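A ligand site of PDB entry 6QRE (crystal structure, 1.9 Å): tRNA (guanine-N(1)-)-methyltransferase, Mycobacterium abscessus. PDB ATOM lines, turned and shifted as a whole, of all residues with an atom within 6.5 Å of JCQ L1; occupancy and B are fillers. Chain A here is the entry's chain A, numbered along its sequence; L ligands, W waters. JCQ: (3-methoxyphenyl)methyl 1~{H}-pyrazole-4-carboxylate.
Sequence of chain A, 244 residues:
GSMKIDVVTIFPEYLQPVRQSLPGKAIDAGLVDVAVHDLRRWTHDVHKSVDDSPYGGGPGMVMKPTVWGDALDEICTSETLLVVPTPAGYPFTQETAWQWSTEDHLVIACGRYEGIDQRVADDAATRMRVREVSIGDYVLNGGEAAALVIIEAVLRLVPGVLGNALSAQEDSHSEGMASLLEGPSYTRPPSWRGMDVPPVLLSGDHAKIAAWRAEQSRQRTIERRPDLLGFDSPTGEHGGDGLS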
ATOM      1  N   VAL A  84      -3.111  -4.205  -3.322  1.00  0.00           N
ATOM      2  CA  VAL A  84      -4.255  -3.619  -4.021  1.00  0.00           C
ATOM      3  C   VAL A  84      -3.824  -2.450  -4.865  1.00  0.00           C
ATOM      4  O   VAL A  84      -3.593  -1.362  -4.346  1.00  0.00           O
ATOM      5  CB  VAL A  84      -5.332  -3.135  -3.045  1.00  0.00           C
ATOM      6  CG1 VAL A  84      -6.580  -2.739  -3.789  1.00  0.00           C
ATOM      7  CG2 VAL A  84      -5.648  -4.222  -2.050  1.00  0.00           C
ATOM      8  N   PRO A  85      -3.683  -2.655  -6.186  1.00  0.00           N
ATOM      9  CA  PRO A  85      -3.271  -1.501  -6.993  1.00  0.00           C
ATOM     10  C   PRO A  85      -4.382  -0.468  -7.074  1.00  0.00           C
ATOM     11  O   PRO A  85      -5.539  -0.841  -7.275  1.00  0.00           O
ATOM     12  CB  PRO A  85      -2.959  -2.103  -8.366  1.00  0.00           C
ATOM     13  CG  PRO A  85      -2.766  -3.620  -8.088  1.00  0.00           C
ATOM     14  CD  PRO A  85      -3.713  -3.906  -6.962  1.00  0.00           C
ATOM     15  N   THR A  86      -4.038   0.804  -6.903  1.00  0.00           N
ATOM     16  CA  THR A  86      -5.022   1.886  -7.010  1.00  0.00           C
ATOM     17  C   THR A  86      -4.288   3.222  -7.130  1.00  0.00           C
ATOM     18  O   THR A  86      -3.243   3.418  -6.509  1.00  0.00           O
ATOM     19  CB  THR A  86      -5.978   1.924  -5.808  1.00  0.00           C
ATOM     20  OG1 THR A  86      -6.671   3.177  -5.764  1.00  0.00           O
ATOM     21  CG2 THR A  86      -5.203   1.760  -4.518  1.00  0.00           C
ATOM     22  N   PRO A  87      -4.830   4.122  -7.927  1.00  0.00           N
ATOM     23  CA  PRO A  87      -4.198   5.445  -8.091  1.00  0.00           C
ATOM     24  C   PRO A  87      -4.214   6.227  -6.783  1.00  0.00           C
ATOM     25  O   PRO A  87      -3.531   7.237  -6.681  1.00  0.00           O
ATOM     26  CB  PRO A  87      -5.054   6.127  -9.175  1.00  0.00           C
ATOM     27  CG  PRO A  87      -6.318   5.354  -9.241  1.00  0.00           C
ATOM     28  CD  PRO A  87      -6.028   3.967  -8.761  1.00  0.00           C
ATOM     29  N   ALA A  88      -4.957   5.767  -5.781  1.00  0.00           N
ATOM     30  CA  ALA A  88      -5.003   6.422  -4.480  1.00  0.00           C
ATOM     31  C   ALA A  88      -4.020   5.796  -3.488  1.00  0.00           C
ATOM     32  O   ALA A  88      -4.093   6.068  -2.298  1.00  0.00           O
ATOM     33  CB  ALA A  88      -6.401   6.376  -3.907  1.00  0.00           C
ATOM     34  N   ALA A 109      -5.181  -8.012  -5.685  1.00  0.00           N
ATOM     35  CA  ALA A 109      -6.595  -7.798  -5.972  1.00  0.00           C
ATOM     36  C   ALA A 109      -6.789  -6.700  -7.005  1.00  0.00           C
ATOM     37  O   ALA A 109      -6.555  -5.522  -6.712  1.00  0.00           O
ATOM     38  CB  ALA A 109      -7.312  -7.442  -4.703  1.00  0.00           C
ATOM     39  N   CYS A 110      -7.210  -7.094  -8.202  1.00  0.00           N
ATOM     40  CA  CYS A 110      -7.445  -6.128  -9.282  1.00  0.00           C
ATOM     41  C   CYS A 110      -8.850  -5.571  -9.205  1.00  0.00           C
ATOM     42  O   CYS A 110      -9.839  -6.292  -9.375  1.00  0.00           O
ATOM     43  CB  CYS A 110      -7.218  -6.761 -10.643  1.00  0.00           C
ATOM     44  SG  CYS A 110      -5.575  -7.434 -10.860  1.00  0.00           S
ATOM     45  N   GLY A 111      -8.920  -4.266  -8.962  1.00  0.00           N
ATOM     46  CA  GLY A 111     -10.172  -3.573  -8.846  1.00  0.00           C
ATOM     47  C   GLY A 111     -10.495  -2.821 -10.114  1.00  0.00           C
ATOM     48  O   GLY A 111      -9.656  -2.677 -10.988  1.00  0.00           O
ATOM     49  N   ARG A 112     -11.733  -2.360 -10.212  1.00  0.00           N
ATOM     50  CA  ARG A 112     -12.158  -1.590 -11.366  1.00  0.00           C
ATOM     51  C   ARG A 112     -12.527  -0.196 -10.910  1.00  0.00           C
ATOM     52  O   ARG A 112     -12.993  -0.001  -9.787  1.00  0.00           O
ATOM     53  CB  ARG A 112     -13.332  -2.271 -12.079  1.00  0.00           C
ATOM     54  CG  ARG A 112     -14.090  -1.376 -13.045  1.00  0.00           C
ATOM     55  CD  ARG A 112     -14.650  -2.164 -14.202  1.00  0.00           C
ATOM     56  NE  ARG A 112     -15.794  -2.975 -13.809  1.00  0.00           N
ATOM     57  CZ  ARG A 112     -16.432  -3.805 -14.630  1.00  0.00           C
ATOM     58  NH1 ARG A 112     -16.009  -3.931 -15.889  1.00  0.00           N
ATOM     59  NH2 ARG A 112     -17.471  -4.514 -14.204  1.00  0.00           N
ATOM     60  N   TYR A 113     -12.302   0.769 -11.806  1.00  0.00           N
ATOM     61  CA  TYR A 113     -12.451   2.177 -11.523  1.00  0.00           C
ATOM     62  C   TYR A 113     -13.651   2.550 -10.647  1.00  0.00           C
ATOM     63  O   TYR A 113     -14.752   2.025 -10.809  1.00  0.00           O
ATOM     64  CB  TYR A 113     -12.520   2.958 -12.842  1.00  0.00           C
ATOM     65  CG  TYR A 113     -12.984   4.381 -12.651  1.00  0.00           C
ATOM     66  CD1 TYR A 113     -12.120   5.343 -12.128  1.00  0.00           C
ATOM     67  CD2 TYR A 113     -14.282   4.759 -12.959  1.00  0.00           C
ATOM     68  CE1 TYR A 113     -12.536   6.641 -11.944  1.00  0.00           C
ATOM     69  CE2 TYR A 113     -14.711   6.052 -12.777  1.00  0.00           C
ATOM     70  CZ  TYR A 113     -13.836   6.993 -12.263  1.00  0.00           C
ATOM     71  OH  TYR A 113     -14.257   8.283 -12.076  1.00  0.00           O
ATOM     72  N   GLU A 114     -13.370   3.545  -9.800  1.00  0.00           N
ATOM     73  CA  GLU A 114     -14.059   3.964  -8.590  1.00  0.00           C
ATOM     74  C   GLU A 114     -13.437   3.217  -7.412  1.00  0.00           C
ATOM     75  O   GLU A 114     -13.069   3.835  -6.419  1.00  0.00           O
ATOM     76  CB  GLU A 114     -15.554   3.746  -8.635  1.00  0.00           C
ATOM     77  CG  GLU A 114     -16.347   4.932  -9.130  1.00  0.00           C
ATOM     78  CD  GLU A 114     -17.006   5.692  -7.998  1.00  0.00           C
ATOM     79  OE1 GLU A 114     -17.856   6.563  -8.294  1.00  0.00           O
ATOM     80  OE2 GLU A 114     -16.690   5.429  -6.822  1.00  0.00           O
ATOM     81  N   GLY A 115     -13.304   1.896  -7.539  1.00  0.00           N
ATOM     82  CA  GLY A 115     -12.540   1.143  -6.561  1.00  0.00           C
ATOM     83  C   GLY A 115     -13.313   0.046  -5.868  1.00  0.00           C
ATOM     84  O   GLY A 115     -14.420  -0.304  -6.270  1.00  0.00           O
ATOM     85  N   ILE A 116     -12.707  -0.500  -4.813  1.00  0.00           N
ATOM     86  CA  ILE A 116     -13.282  -1.592  -4.034  1.00  0.00           C
ATOM     87  C   ILE A 116     -13.772  -1.043  -2.710  1.00  0.00           C
ATOM     88  O   ILE A 116     -13.090  -0.255  -2.080  1.00  0.00           O
ATOM     89  CB  ILE A 116     -12.235  -2.685  -3.789  1.00  0.00           C
ATOM     90  CG1 ILE A 116     -11.649  -3.161  -5.118  1.00  0.00           C
ATOM     91  CG2 ILE A 116     -12.818  -3.832  -2.921  1.00  0.00           C
ATOM     92  CD1 ILE A 116     -10.517  -4.160  -4.958  1.00  0.00           C
ATOM     93  N   VAL A 133      -1.293   0.346  -3.278  1.00  0.00           N
ATOM     94  CA  VAL A 133      -0.182   1.023  -3.927  1.00  0.00           C
ATOM     95  C   VAL A 133      -0.547   1.543  -5.311  1.00  0.00           C
ATOM     96  O   VAL A 133      -1.417   1.001  -5.998  1.00  0.00           O
ATOM     97  CB  VAL A 133       1.045   0.104  -4.053  1.00  0.00           C
ATOM     98  CG1 VAL A 133       1.562  -0.267  -2.676  1.00  0.00           C
ATOM     99  CG2 VAL A 133       0.683  -1.160  -4.840  1.00  0.00           C
ATOM    100  N   SER A 134       0.102   2.629  -5.696  1.00  0.00           N
ATOM    101  CA  SER A 134      -0.048   3.191  -7.033  1.00  0.00           C
ATOM    102  C   SER A 134       1.232   2.954  -7.806  1.00  0.00           C
ATOM    103  O   SER A 134       2.312   3.178  -7.272  1.00  0.00           O
ATOM    104  CB  SER A 134      -0.362   4.692  -6.974  1.00  0.00           C
ATOM    105  OG  SER A 134      -0.147   5.302  -8.239  1.00  0.00           O
ATOM    106  N   ILE A 135       1.123   2.533  -9.055  1.00  0.00           N
ATOM    107  CA  ILE A 135       2.313   2.370  -9.879  1.00  0.00           C
ATOM    108  C   ILE A 135       2.622   3.660 -10.666  1.00  0.00           C
ATOM    109  O   ILE A 135       3.590   3.727 -11.419  1.00  0.00           O
ATOM    110  CB  ILE A 135       2.186   1.221 -10.876  1.00  0.00           C
ATOM    111  CG1 ILE A 135       0.997   1.449 -11.809  1.00  0.00           C
ATOM    112  CG2 ILE A 135       2.059  -0.129 -10.139  1.00  0.00           C
ATOM    113  CD1 ILE A 135       1.127   0.710 -13.109  1.00  0.00           C
ATOM    114  N   GLY A 136       1.788   4.694 -10.506  1.00  0.00           N
ATOM    115  CA  GLY A 136       1.954   5.904 -11.282  1.00  0.00           C
ATOM    116  C   GLY A 136       0.754   6.809 -11.235  1.00  0.00           C
ATOM    117  O   GLY A 136      -0.372   6.379 -10.973  1.00  0.00           O
ATOM    118  N   ASP A 137       0.983   8.095 -11.470  1.00  0.00           N
ATOM    119  CA  ASP A 137      -0.073   9.089 -11.362  1.00  0.00           C
ATOM    120  C   ASP A 137      -0.898   9.193 -12.631  1.00  0.00           C
ATOM    121  O   ASP A 137      -0.817  10.176 -13.372  1.00  0.00           O
ATOM    122  CB  ASP A 137       0.507  10.462 -11.016  1.00  0.00           C
ATOM    123  CG  ASP A 137       0.922  10.550  -9.561  1.00  0.00           C
ATOM    124  OD1 ASP A 137       0.418   9.747  -8.747  1.00  0.00           O
ATOM    125  OD2 ASP A 137       1.732  11.420  -9.228  1.00  0.00           O
ATOM    126  N   TYR A 138      -1.700   8.169 -12.861  1.00  0.00           N
ATOM    127  CA  TYR A 138      -2.631   8.150 -13.976  1.00  0.00           C
ATOM    128  C   TYR A 138      -3.773   7.221 -13.577  1.00  0.00           C
ATOM    129  O   TYR A 138      -3.666   6.507 -12.579  1.00  0.00           O
ATOM    130  CB  TYR A 138      -1.930   7.692 -15.258  1.00  0.00           C
ATOM    131  CG  TYR A 138      -0.854   6.656 -15.005  1.00  0.00           C
ATOM    132  CD1 TYR A 138      -1.180   5.341 -14.689  1.00  0.00           C
ATOM    133  CD2 TYR A 138       0.487   7.010 -15.051  1.00  0.00           C
ATOM    134  CE1 TYR A 138      -0.191   4.392 -14.429  1.00  0.00           C
ATOM    135  CE2 TYR A 138       1.493   6.069 -14.812  1.00  0.00           C
ATOM    136  CZ  TYR A 138       1.145   4.768 -14.492  1.00  0.00           C
ATOM    137  OH  TYR A 138       2.127   3.848 -14.226  1.00  0.00           O
ATOM    138  N   VAL A 139      -4.862   7.239 -14.329  1.00  0.00           N
ATOM    139  CA  VAL A 139      -5.996   6.358 -14.041  1.00  0.00           C
ATOM    140  C   VAL A 139      -6.109   5.298 -15.119  1.00  0.00           C
ATOM    141  O   VAL A 139      -6.054   5.628 -16.309  1.00  0.00           O
ATOM    142  CB  VAL A 139      -7.328   7.123 -13.957  1.00  0.00           C
ATOM    143  CG1 VAL A 139      -8.495   6.158 -13.614  1.00  0.00           C
ATOM    144  CG2 VAL A 139      -7.241   8.229 -12.943  1.00  0.00           C
ATOM    145  N   LEU A 140      -6.246   4.033 -14.699  1.00  0.00           N
ATOM    146  CA  LEU A 140      -6.542   2.924 -15.603  1.00  0.00           C
ATOM    147  C   LEU A 140      -7.988   2.467 -15.376  1.00  0.00           C
ATOM    148  O   LEU A 140      -8.576   2.779 -14.343  1.00  0.00           O
ATOM    149  CB  LEU A 140      -5.569   1.767 -15.359  1.00  0.00           C
ATOM    150  CG  LEU A 140      -4.091   2.173 -15.228  1.00  0.00           C
ATOM    151  CD1 LEU A 140      -3.203   0.991 -14.862  1.00  0.00           C
ATOM    152  CD2 LEU A 140      -3.641   2.778 -16.536  1.00  0.00           C
ATOM    153  N   ASN A 141      -8.558   1.711 -16.305  1.00  0.00           N
ATOM    154  CA  ASN A 141      -9.927   1.193 -16.091  1.00  0.00           C
ATOM    155  C   ASN A 141      -9.961   0.047 -15.108  1.00  0.00           C
ATOM    156  O   ASN A 141     -10.993  -0.218 -14.477  1.00  0.00           O
ATOM    157  CB  ASN A 141     -10.540   0.747 -17.406  1.00  0.00           C
ATOM    158  CG  ASN A 141     -11.345   1.847 -18.073  1.00  0.00           C
ATOM    159  OD1 ASN A 141     -11.688   2.848 -17.431  1.00  0.00           O
ATOM    160  ND2 ASN A 141     -11.647   1.669 -19.357  1.00  0.00           N
ATOM    161  N   GLY A 142      -8.841  -0.655 -14.972  1.00  0.00           N
ATOM    162  CA  GLY A 142      -8.717  -1.732 -14.010  1.00  0.00           C
ATOM    163  C   GLY A 142      -7.290  -1.898 -13.519  1.00  0.00           C
ATOM    164  O   GLY A 142      -6.344  -1.356 -14.099  1.00  0.00           O
ATOM    165  N   GLY A 143      -7.139  -2.636 -12.434  1.00  0.00           N
ATOM    166  CA  GLY A 143      -5.825  -2.889 -11.850  1.00  0.00           C
ATOM    167  C   GLY A 143      -4.963  -3.896 -12.589  1.00  0.00           C
ATOM    168  O   GLY A 143      -3.785  -4.075 -12.241  1.00  0.00           O
ATOM    169  N   GLU A 144      -5.517  -4.544 -13.609  1.00  0.00           N
ATOM    170  CA  GLU A 144      -4.822  -5.656 -14.260  1.00  0.00           C
ATOM    171  C   GLU A 144      -3.442  -5.270 -14.845  1.00  0.00           C
ATOM    172  O   GLU A 144      -2.474  -5.982 -14.629  1.00  0.00           O
ATOM    173  CB  GLU A 144      -5.704  -6.245 -15.367  1.00  0.00           C
ATOM    174  CG  GLU A 144      -6.882  -7.096 -14.842  1.00  0.00           C
ATOM    175  CD  GLU A 144      -8.025  -6.262 -14.287  1.00  0.00           C
ATOM    176  OE1 GLU A 144      -8.030  -5.022 -14.488  1.00  0.00           O
ATOM    177  OE2 GLU A 144      -8.927  -6.835 -13.641  1.00  0.00           O
ATOM    178  N   ALA A 146      -1.592  -2.801 -13.934  1.00  0.00           N
ATOM    179  CA  ALA A 146      -0.743  -2.510 -12.776  1.00  0.00           C
ATOM    180  C   ALA A 146      -0.222  -3.797 -12.136  1.00  0.00           C
ATOM    181  O   ALA A 146       0.923  -3.865 -11.667  1.00  0.00           O
ATOM    182  CB  ALA A 146      -1.493  -1.657 -11.755  1.00  0.00           C
HETATM  183  C10 JCQ L   1      -2.743   1.880 -10.171  1.00  0.00           C
HETATM  184  N12 JCQ L   1      -1.792   3.791 -10.719  1.00  0.00           N
HETATM  185  C13 JCQ L   1      -3.009   3.753 -11.341  1.00  0.00           C
HETATM  186  C15 JCQ L   1      -8.524   2.429 -10.702  1.00  0.00           C
HETATM  187  C17 JCQ L   1      -9.677   2.446  -8.559  1.00  0.00           C
HETATM  188  C01 JCQ L   1      -8.788  -0.593  -6.790  1.00  0.00           C
HETATM  189  O02 JCQ L   1      -9.316   0.676  -6.947  1.00  0.00           O
HETATM  190  C03 JCQ L   1      -9.057   1.280  -8.225  1.00  0.00           C
HETATM  191  C04 JCQ L   1      -8.146   0.667  -9.111  1.00  0.00           C
HETATM  192  C05 JCQ L   1      -7.885   1.245 -10.349  1.00  0.00           C
HETATM  193  C06 JCQ L   1      -6.921   0.612 -11.285  1.00  0.00           C
HETATM  194  O07 JCQ L   1      -5.561   0.909 -10.850  1.00  0.00           O
HETATM  195  C08 JCQ L   1      -5.004   2.075 -11.441  1.00  0.00           C
HETATM  196  C09 JCQ L   1      -3.609   2.557 -10.993  1.00  0.00           C
HETATM  197  N11 JCQ L   1      -1.665   2.628 -10.022  1.00  0.00           N
HETATM  198  O14 JCQ L   1      -5.643   2.712 -12.277  1.00  0.00           O
HETATM  199  C16 JCQ L   1      -9.423   3.035  -9.818  1.00  0.00           C
HETATM  200  C10 JCQ L   2      -9.417   6.500  -7.455  1.00  0.00           C
HETATM  201  N12 JCQ L   2     -10.342   6.809  -9.443  1.00  0.00           N
HETATM  202  C13 JCQ L   2      -9.383   7.757  -9.292  1.00  0.00           C
HETATM  203  C15 JCQ L   2      -5.253   9.945 -10.331  1.00  0.00           C
HETATM  204  C17 JCQ L   2      -3.293  11.114 -11.165  1.00  0.00           C
HETATM  205  C01 JCQ L   2      -1.999  13.271  -8.752  1.00  0.00           C
HETATM  206  O02 JCQ L   2      -1.784  12.209  -9.625  1.00  0.00           O
HETATM  207  C03 JCQ L   2      -2.954  11.447  -9.888  1.00  0.00           C
HETATM  208  C04 JCQ L   2      -3.761  11.033  -8.807  1.00  0.00           C
HETATM  209  C05 JCQ L   2      -4.905  10.288  -9.042  1.00  0.00           C
HETATM  210  C06 JCQ L   2      -5.757   9.861  -7.888  1.00  0.00           C
HETATM  211  O07 JCQ L   2      -6.902   9.179  -8.410  1.00  0.00           O
HETATM  212  C08 JCQ L   2      -7.654   8.406  -7.488  1.00  0.00           C
HETATM  213  C09 JCQ L   2      -8.797   7.568  -8.059  1.00  0.00           C
HETATM  214  N11 JCQ L   2     -10.338   6.063  -8.303  1.00  0.00           N
HETATM  215  O14 JCQ L   2      -7.411   8.432  -6.274  1.00  0.00           O
HETATM  216  C16 JCQ L   2      -4.450  10.351 -11.409  1.00  0.00           C
HETATM  217  O   HOH W   1     -10.192   0.697  -3.685  1.00  0.00           O
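The backbone carbonyl oxygen (O) of Ile 135 lies within hydrogen-bond range of the side-chain hydroxyl (OH) of Tyr 138, 3.2 Å away.
The side-chain hydroxyl (OG) of Ser 134 lies within hydrogen-bond range of the backbone carbonyl oxygen (O) of Gly 136, at 2.9 Å.
O of Gly 111 lies within hydrogen-bond range of N of Gly 143 (2.9 Å).
The backbone NH of Tyr 113 lies within hydrogen-bond range of the backbone carbonyl oxygen of Asn 141.
The backbone NH of Thr 86 is in hydrogen-bond range of the backbone carbonyl oxygen of Val 133, 2.8 Å away.
The backbone NH (N) of Ala 88 lies close to the side-chain hydroxyl (OG1) of Thr 86 (3.1 Å).
N of Leu 140 is in hydrogen-bond range of O14 of JCQ L1, 2.8 Å away.
N of Ile 135 sits at hydrogen-bond distance from N11 of JCQ L1 (3.0 Å).
The backbone carbonyl oxygen of Gly 136 lies within hydrogen-bond range of a nitrogen (N12) of JCQ L1 (3.0 Å).
N12 of JCQ L1 lies within hydrogen-bond range of OG of Ser 134 (3.3 Å).
Merely in contact with JCQ L1: Tyr 138 (3.1 Å), Gly 115 (3.3 Å), Pro 85 (3.3 Å), Gly 142 (3.4 Å), Pro 87 (3.4 Å), Gly 143 (3.5 Å), Tyr 113 (3.6 Å), Thr 86 (3.7 Å), Val 139 (3.9 Å), Gly 111 (3.9 Å) and Glu 114 (3.98 Å).
Hydrophobic or aromatic side chains that line JCQ L1: Pro 87, Ile 135 and Leu 140.
Of the 26 residues printed, 15 come within 4 Å of JCQ L1.
The nearest printed residue that does not touch JCQ L1 is Ala 146 (4.1 Å).
Water W1 bridges N of Ile 116 (3.0 Å) and O02 of JCQ L1 (3.4 Å).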
